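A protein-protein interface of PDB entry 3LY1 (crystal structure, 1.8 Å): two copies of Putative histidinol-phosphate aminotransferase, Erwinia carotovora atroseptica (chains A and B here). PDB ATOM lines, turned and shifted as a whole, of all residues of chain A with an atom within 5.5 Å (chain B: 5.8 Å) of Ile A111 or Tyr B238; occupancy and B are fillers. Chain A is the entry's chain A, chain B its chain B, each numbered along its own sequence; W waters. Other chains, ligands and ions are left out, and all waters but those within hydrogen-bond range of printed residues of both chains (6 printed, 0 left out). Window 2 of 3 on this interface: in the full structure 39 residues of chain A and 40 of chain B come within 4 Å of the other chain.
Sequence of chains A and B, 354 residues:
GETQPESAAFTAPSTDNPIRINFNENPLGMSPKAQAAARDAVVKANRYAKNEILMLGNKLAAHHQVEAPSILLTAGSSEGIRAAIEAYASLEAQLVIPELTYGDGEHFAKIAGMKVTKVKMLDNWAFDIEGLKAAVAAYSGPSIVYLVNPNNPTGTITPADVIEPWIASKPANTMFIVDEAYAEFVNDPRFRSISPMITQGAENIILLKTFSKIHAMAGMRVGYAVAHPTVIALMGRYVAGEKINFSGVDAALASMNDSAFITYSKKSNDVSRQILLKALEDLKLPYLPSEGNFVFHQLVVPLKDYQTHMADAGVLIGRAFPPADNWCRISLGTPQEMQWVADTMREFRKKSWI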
ATOM      1  N   GLU A  79      -1.816 -19.758  18.011  1.00  0.00           N
ATOM      2  CA  GLU A  79      -0.552 -19.262  17.459  1.00  0.00           C
ATOM      3  C   GLU A  79      -0.673 -18.756  16.029  1.00  0.00           C
ATOM      4  O   GLU A  79      -0.004 -17.794  15.662  1.00  0.00           O
ATOM      5  CB  GLU A  79       0.596 -20.268  17.616  1.00  0.00           C
ATOM      6  CG  GLU A  79       1.060 -20.473  19.082  1.00  0.00           C
ATOM      7  CD  GLU A  79       1.720 -19.261  19.747  1.00  0.00           C
ATOM      8  OE1 GLU A  79       1.924 -18.179  19.127  1.00  0.00           O
ATOM      9  OE2 GLU A  79       2.084 -19.402  20.951  1.00  0.00           O
ATOM     10  N   ARG A  82      -2.160 -15.150  16.326  1.00  0.00           N
ATOM     11  CA  ARG A  82      -1.020 -14.292  16.672  1.00  0.00           C
ATOM     12  C   ARG A  82      -0.129 -13.994  15.477  1.00  0.00           C
ATOM     13  O   ARG A  82       0.134 -12.841  15.169  1.00  0.00           O
ATOM     14  CB  ARG A  82      -0.192 -14.856  17.839  1.00  0.00           C
ATOM     15  CG  ARG A  82       0.863 -13.828  18.313  1.00  0.00           C
ATOM     16  CD  ARG A  82       1.874 -14.401  19.326  1.00  0.00           C
ATOM     17  NE  ARG A  82       2.454 -15.622  18.803  1.00  0.00           N
ATOM     18  CZ  ARG A  82       3.355 -15.681  17.839  1.00  0.00           C
ATOM     19  NH1 ARG A  82       3.845 -14.575  17.242  1.00  0.00           N
ATOM     20  NH2 ARG A  82       3.748 -16.853  17.428  1.00  0.00           N
ATOM     21  N   GLU A  86       0.528 -10.428  13.708  1.00  0.00           N
ATOM     22  CA  GLU A  86       1.884  -9.838  13.717  1.00  0.00           C
ATOM     23  C   GLU A  86       2.395  -9.580  12.294  1.00  0.00           C
ATOM     24  O   GLU A  86       3.072  -8.571  12.018  1.00  0.00           O
ATOM     25  CB  GLU A  86       2.860 -10.735  14.529  1.00  0.00           C
ATOM     26  CG  GLU A  86       2.653 -10.623  16.062  1.00  0.00           C
ATOM     27  CD  GLU A  86       3.744 -11.354  16.860  1.00  0.00           C
ATOM     28  OE1 GLU A  86       4.846 -11.557  16.314  1.00  0.00           O
ATOM     29  OE2 GLU A  86       3.498 -11.724  18.016  1.00  0.00           O
ATOM     30  N   GLU A 106      -8.476  -9.091  18.787  1.00  0.00           N
ATOM     31  CA  GLU A 106      -8.363  -7.806  19.472  1.00  0.00           C
ATOM     32  C   GLU A 106      -7.100  -7.732  20.384  1.00  0.00           C
ATOM     33  O   GLU A 106      -6.389  -6.699  20.428  1.00  0.00           O
ATOM     34  CB  GLU A 106      -9.652  -7.530  20.260  1.00  0.00           C
ATOM     35  CG  GLU A 106      -9.533  -6.497  21.309  1.00  0.00           C
ATOM     36  CD  GLU A 106     -10.872  -6.128  21.940  1.00  0.00           C
ATOM     37  OE1 GLU A 106     -11.788  -6.965  21.999  1.00  0.00           O
ATOM     38  OE2 GLU A 106     -10.987  -4.994  22.410  1.00  0.00           O
ATOM     39  N   HIS A 107      -6.881  -8.802  21.129  1.00  0.00           N
ATOM     40  CA  HIS A 107      -5.767  -8.934  22.067  1.00  0.00           C
ATOM     41  C   HIS A 107      -4.426  -8.688  21.382  1.00  0.00           C
ATOM     42  O   HIS A 107      -3.624  -7.853  21.857  1.00  0.00           O
ATOM     43  CB  HIS A 107      -5.804 -10.328  22.721  1.00  0.00           C
ATOM     44  CG  HIS A 107      -4.607 -10.650  23.562  1.00  0.00           C
ATOM     45  ND1 HIS A 107      -4.493 -10.270  24.880  1.00  0.00           N
ATOM     46  CD2 HIS A 107      -3.490 -11.377  23.285  1.00  0.00           C
ATOM     47  CE1 HIS A 107      -3.333 -10.691  25.358  1.00  0.00           C
ATOM     48  NE2 HIS A 107      -2.707 -11.368  24.413  1.00  0.00           N
ATOM     49  N   PHE A 108      -4.162  -9.415  20.289  1.00  0.00           N
ATOM     50  CA  PHE A 108      -2.909  -9.265  19.561  1.00  0.00           C
ATOM     51  C   PHE A 108      -2.890  -7.956  18.781  1.00  0.00           C
ATOM     52  O   PHE A 108      -1.817  -7.338  18.586  1.00  0.00           O
ATOM     53  CB  PHE A 108      -2.631 -10.493  18.664  1.00  0.00           C
ATOM     54  CG  PHE A 108      -2.449 -11.779  19.439  1.00  0.00           C
ATOM     55  CD1 PHE A 108      -1.397 -11.931  20.336  1.00  0.00           C
ATOM     56  CD2 PHE A 108      -3.330 -12.818  19.293  1.00  0.00           C
ATOM     57  CE1 PHE A 108      -1.271 -13.089  21.086  1.00  0.00           C
ATOM     58  CE2 PHE A 108      -3.168 -13.981  20.023  1.00  0.00           C
ATOM     59  CZ  PHE A 108      -2.142 -14.094  20.915  1.00  0.00           C
ATOM     60  N   ALA A 109      -4.068  -7.473  18.375  1.00  0.00           N
ATOM     61  CA  ALA A 109      -4.122  -6.177  17.688  1.00  0.00           C
ATOM     62  C   ALA A 109      -3.718  -5.018  18.596  1.00  0.00           C
ATOM     63  O   ALA A 109      -2.969  -4.089  18.190  1.00  0.00           O
ATOM     64  CB  ALA A 109      -5.536  -5.942  17.034  1.00  0.00           C
ATOM     65  N   LYS A 110      -4.184  -5.075  19.829  1.00  0.00           N
ATOM     66  CA  LYS A 110      -3.800  -4.111  20.853  1.00  0.00           C
ATOM     67  C   LYS A 110      -2.295  -4.139  21.196  1.00  0.00           C
ATOM     68  O   LYS A 110      -1.690  -3.099  21.341  1.00  0.00           O
ATOM     69  CB  LYS A 110      -4.620  -4.323  22.100  1.00  0.00           C
ATOM     70  CG  LYS A 110      -6.062  -3.865  21.942  1.00  0.00           C
ATOM     71  CD  LYS A 110      -6.702  -3.531  23.315  1.00  0.00           C
ATOM     72  CE  LYS A 110      -7.355  -4.719  23.940  1.00  0.00           C
ATOM     73  NZ  LYS A 110      -7.694  -4.499  25.426  1.00  0.00           N
ATOM     74  N   ILE A 111      -1.717  -5.324  21.323  1.00  0.00           N
ATOM     75  CA  ILE A 111      -0.264  -5.486  21.500  1.00  0.00           C
ATOM     76  C   ILE A 111       0.495  -4.804  20.364  1.00  0.00           C
ATOM     77  O   ILE A 111       1.467  -4.084  20.605  1.00  0.00           O
ATOM     78  CB  ILE A 111       0.094  -7.000  21.675  1.00  0.00           C
ATOM     79  CG1 ILE A 111      -0.377  -7.488  23.057  1.00  0.00           C
ATOM     80  CG2 ILE A 111       1.580  -7.256  21.470  1.00  0.00           C
ATOM     81  CD1 ILE A 111      -0.658  -8.975  23.137  1.00  0.00           C
ATOM     82  N   ALA A 112      -0.008  -4.942  19.131  1.00  0.00           N
ATOM     83  CA  ALA A 112       0.575  -4.288  17.968  1.00  0.00           C
ATOM     84  C   ALA A 112       0.313  -2.765  17.883  1.00  0.00           C
ATOM     85  O   ALA A 112       0.873  -2.054  17.015  1.00  0.00           O
ATOM     86  CB  ALA A 112       0.103  -5.024  16.669  1.00  0.00           C
ATOM     87  N   GLY A 113      -0.500  -2.236  18.785  1.00  0.00           N
ATOM     88  CA  GLY A 113      -0.740  -0.779  18.804  1.00  0.00           C
ATOM     89  C   GLY A 113      -1.728  -0.339  17.733  1.00  0.00           C
ATOM     90  O   GLY A 113      -1.820   0.830  17.417  1.00  0.00           O
ATOM     91  N   ARG B  82      12.478 -16.277  20.208  1.00  0.00           N
ATOM     92  CA  ARG B  82      11.654 -15.415  19.346  1.00  0.00           C
ATOM     93  C   ARG B  82      10.950 -14.314  20.147  1.00  0.00           C
ATOM     94  O   ARG B  82      11.011 -13.138  19.788  1.00  0.00           O
ATOM     95  CB  ARG B  82      10.607 -16.224  18.575  1.00  0.00           C
ATOM     96  CG  ARG B  82       9.830 -15.362  17.586  1.00  0.00           C
ATOM     97  CD  ARG B  82       8.676 -16.075  16.895  1.00  0.00           C
ATOM     98  NE  ARG B  82       7.805 -16.700  17.876  1.00  0.00           N
ATOM     99  CZ  ARG B  82       6.969 -16.060  18.685  1.00  0.00           C
ATOM    100  NH1 ARG B  82       6.837 -14.738  18.637  1.00  0.00           N
ATOM    101  NH2 ARG B  82       6.267 -16.772  19.563  1.00  0.00           N
ATOM    102  N   ALA B  83      10.329 -14.701  21.253  1.00  0.00           N
ATOM    103  CA  ALA B  83       9.555 -13.779  22.104  1.00  0.00           C
ATOM    104  C   ALA B  83      10.455 -12.740  22.751  1.00  0.00           C
ATOM    105  O   ALA B  83      10.093 -11.520  22.808  1.00  0.00           O
ATOM    106  CB  ALA B  83       8.767 -14.598  23.164  1.00  0.00           C
ATOM    107  N   GLU B  86      11.363 -10.354  19.913  1.00  0.00           N
ATOM    108  CA  GLU B  86      10.228  -9.506  19.546  1.00  0.00           C
ATOM    109  C   GLU B  86       9.904  -8.458  20.615  1.00  0.00           C
ATOM    110  O   GLU B  86       9.516  -7.342  20.285  1.00  0.00           O
ATOM    111  CB  GLU B  86       8.988 -10.313  19.163  1.00  0.00           C
ATOM    112  CG  GLU B  86       9.193 -11.158  17.879  1.00  0.00           C
ATOM    113  CD  GLU B  86       7.911 -11.795  17.360  1.00  0.00           C
ATOM    114  OE1 GLU B  86       6.817 -11.336  17.741  1.00  0.00           O
ATOM    115  OE2 GLU B  86       8.001 -12.762  16.573  1.00  0.00           O
ATOM    116  N   ALA B  87      10.035  -8.833  21.882  1.00  0.00           N
ATOM    117  CA  ALA B  87       9.698  -7.955  22.982  1.00  0.00           C
ATOM    118  C   ALA B  87      10.624  -6.749  23.067  1.00  0.00           C
ATOM    119  O   ALA B  87      10.179  -5.712  23.519  1.00  0.00           O
ATOM    120  CB  ALA B  87       9.711  -8.716  24.314  1.00  0.00           C
ATOM    121  N   LEU B 234       6.368  -8.456  29.306  1.00  0.00           N
ATOM    122  CA  LEU B 234       6.594  -7.956  27.944  1.00  0.00           C
ATOM    123  C   LEU B 234       6.728  -9.117  26.973  1.00  0.00           C
ATOM    124  O   LEU B 234       6.135  -9.099  25.897  1.00  0.00           O
ATOM    125  CB  LEU B 234       7.838  -7.064  27.836  1.00  0.00           C
ATOM    126  CG  LEU B 234       7.678  -5.633  28.344  1.00  0.00           C
ATOM    127  CD1 LEU B 234       8.935  -4.798  28.034  1.00  0.00           C
ATOM    128  CD2 LEU B 234       6.431  -5.021  27.720  1.00  0.00           C
ATOM    129  N   MET B 235       7.515 -10.134  27.359  1.00  0.00           N
ATOM    130  CA  MET B 235       7.716 -11.343  26.529  1.00  0.00           C
ATOM    131  C   MET B 235       6.427 -12.092  26.277  1.00  0.00           C
ATOM    132  O   MET B 235       6.205 -12.587  25.178  1.00  0.00           O
ATOM    133  CB  MET B 235       8.690 -12.327  27.165  1.00  0.00           C
ATOM    134  CG  MET B 235      10.095 -11.818  27.139  1.00  0.00           C
ATOM    135  SD  MET B 235      11.302 -13.159  27.911  1.00  0.00           S
ATOM    136  CE  MET B 235      11.004 -14.655  26.721  1.00  0.00           C
ATOM    137  N   GLY B 236       5.577 -12.135  27.298  1.00  0.00           N
ATOM    138  CA  GLY B 236       4.270 -12.767  27.202  1.00  0.00           C
ATOM    139  C   GLY B 236       3.337 -12.202  26.135  1.00  0.00           C
ATOM    140  O   GLY B 236       2.396 -12.874  25.727  1.00  0.00           O
ATOM    141  N   ARG B 237       3.566 -10.955  25.719  1.00  0.00           N
ATOM    142  CA  ARG B 237       2.730 -10.337  24.680  1.00  0.00           C
ATOM    143  C   ARG B 237       3.060 -10.863  23.265  1.00  0.00           C
ATOM    144  O   ARG B 237       2.348 -10.570  22.305  1.00  0.00           O
ATOM    145  CB  ARG B 237       2.846  -8.810  24.760  1.00  0.00           C
ATOM    146  CG  ARG B 237       2.351  -8.243  26.109  1.00  0.00           C
ATOM    147  CD  ARG B 237       2.905  -6.831  26.396  1.00  0.00           C
ATOM    148  NE  ARG B 237       2.263  -5.766  25.639  1.00  0.00           N
ATOM    149  CZ  ARG B 237       1.095  -5.216  25.950  1.00  0.00           C
ATOM    150  NH1 ARG B 237       0.408  -5.653  27.000  1.00  0.00           N
ATOM    151  NH2 ARG B 237       0.604  -4.250  25.187  1.00  0.00           N
ATOM    152  N   TYR B 238       4.127 -11.668  23.143  1.00  0.00           N
ATOM    153  CA  TYR B 238       4.546 -12.207  21.858  1.00  0.00           C
ATOM    154  C   TYR B 238       4.459 -13.718  21.771  1.00  0.00           C
ATOM    155  O   TYR B 238       5.010 -14.298  20.865  1.00  0.00           O
ATOM    156  CB  TYR B 238       5.924 -11.699  21.539  1.00  0.00           C
ATOM    157  CG  TYR B 238       5.880 -10.230  21.490  1.00  0.00           C
ATOM    158  CD1 TYR B 238       5.366  -9.592  20.393  1.00  0.00           C
ATOM    159  CD2 TYR B 238       6.223  -9.472  22.590  1.00  0.00           C
ATOM    160  CE1 TYR B 238       5.285  -8.216  20.344  1.00  0.00           C
ATOM    161  CE2 TYR B 238       6.121  -8.079  22.551  1.00  0.00           C
ATOM    162  CZ  TYR B 238       5.645  -7.476  21.442  1.00  0.00           C
ATOM    163  OH  TYR B 238       5.545  -6.102  21.407  1.00  0.00           O
ATOM    164  N   VAL B 239       3.743 -14.333  22.709  1.00  0.00           N
ATOM    165  CA  VAL B 239       3.318 -15.735  22.597  1.00  0.00           C
ATOM    166  C   VAL B 239       1.796 -15.794  22.801  1.00  0.00           C
ATOM    167  O   VAL B 239       1.209 -14.854  23.375  1.00  0.00           O
ATOM    168  CB  VAL B 239       4.035 -16.695  23.617  1.00  0.00           C
ATOM    169  CG1 VAL B 239       5.531 -16.803  23.341  1.00  0.00           C
ATOM    170  CG2 VAL B 239       3.711 -16.360  25.118  1.00  0.00           C
ATOM    171  N   ALA B 240       1.159 -16.869  22.321  1.00  0.00           N
ATOM    172  CA  ALA B 240      -0.292 -17.042  22.442  1.00  0.00           C
ATOM    173  C   ALA B 240      -0.602 -17.713  23.777  1.00  0.00           C
ATOM    174  O   ALA B 240      -1.087 -18.864  23.827  1.00  0.00           O
ATOM    175  CB  ALA B 240      -0.899 -17.876  21.234  1.00  0.00           C
HETATM  176  O   HOH W   1       1.153  -2.247  22.832  1.00  0.00           O
HETATM  177  O   HOH W   2       4.755 -19.093  20.733  1.00  0.00           O
HETATM  178  O   HOH W   3       1.715 -10.518  19.690  1.00  0.00           O
HETATM  179  O   HOH W   4       0.655 -20.833  22.727  1.00  0.00           O
HETATM  180  O   HOH W   5       3.950  -5.130  19.344  1.00  0.00           O
HETATM  181  O   HOH W   6      -0.117 -12.430  24.379  1.00  0.00           O
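Among the printed residues, pairs that only touch across the chains: Arg A82 with Tyr B238 (3.5 Å), Ile A111 with Arg B237 (3.5 Å), Glu A86 with Tyr B238 (3.7 Å), Arg A82 with Val B239 (3.7 Å), Phe A108 with Ala B240 (3.8 Å), Phe A108 with Val B239 (3.8 Å), Arg A82 with Ala B240 (3.9 Å) and Ile A111 with Tyr B238 (3.99 Å).
Water W3 lies within hydrogen-bond range of the backbone carbonyl oxygen of Arg B237 (2.7 Å) and the side-chain carboxylate of Glu A86 (2.7 Å). Water W4 bridges OE2 of Glu A79 (2.7 Å) and O of Ala B240 (2.8 Å). Water W2 lies within hydrogen-bond range of the side-chain carboxylate (OE2) of Glu A79 (2.7 Å) and the guanidinium group (NH2) of Arg B82 (3.0 Å). Water W5 lies within hydrogen-bond range of the side-chain hydroxyl (OH) of Tyr B238 (2.8 Å) and the backbone carbonyl oxygen (O) of Ile A111 (3.0 Å). Water W6 lies within hydrogen-bond range of NE2 of His A107 (2.8 Å), O of Gly B236 (2.9 Å) and O of Val B239 (2.9 Å). Water W1 lies within hydrogen-bond range of O of Ile A111 (2.9 Å), NH2 of Arg B237 (3.1 Å) and O of Lys A110 (3.3 Å).
The side-chain carboxylate (OE1) of Glu A79 is in salt-bridge range of the guanidinium group (NE) of Arg A82, 2.6 Å away. The guanidinium group (NH1) of Arg A82 lies within salt-bridge range of the side-chain carboxylate (OE2) of Glu A86. NH1 of Arg B82 is in salt-bridge range of OE2 of Glu B86 (3.1 Å). O of Tyr B238 sits at hydrogen-bond distance from NH1 of Arg B82 (2.9 Å).
Arg A82 touches its own counterpart, Arg B82. Glu B86 touches its own counterpart, Glu A86. Positions printed for both chains: 82 and 86.
Of the 11 printed residues of chain B, 6 touch a printed residue of chain A. Hydrophobic or aromatic side chains of chain B within 4 Å of the printed part of chain A: Tyr B238 and Ala B240. Of the 11 printed residues of chain A, 5 touch a printed residue of chain B. Hydrophobic or aromatic side chains of chain A within 4 Å of the printed part of chain B: Phe A108 and Ile A111. Along chain A the printed residues that touch a printed residue of chain B span positions 79 to 111. Among the printed residues, 11 pairs touch across the chains. Among the printed residues, no Asp or Glu carboxylate lies within 4 Å of a Lys or Arg side-chain nitrogen of the other chain.
Of the printed residues of chain B, Arg A82 touches Arg B82, Tyr B238, Val B239 and Ala B240. Of the printed residues of chain B, Ile A111 touches Arg B237 (3.5 Å) and Tyr B238 (3.99 Å). Printed residues of chain A within 4 Å of Arg B82: Arg A82. Of the printed residues of chain A, Tyr B238 touches Arg A82, Glu A86 and Ile A111. Printed residues of chain A within 4 Å of Ala B240: Glu A79 (3.0 Å), Arg A82 (3.9 Å) and Phe A108 (3.8 Å). The nearest printed residue of chain B that does not touch Phe A108 is Arg B237 (4.4 Å).
N of Ala B240 sits at hydrogen-bond distance from OE2 of Glu A79. OE1 of Glu B86 sits close to OE1 of Glu A86 (2.4 Å). The guanidinium group of Arg A82 sits close to the guanidinium group of Arg B82 (3.3 Å).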
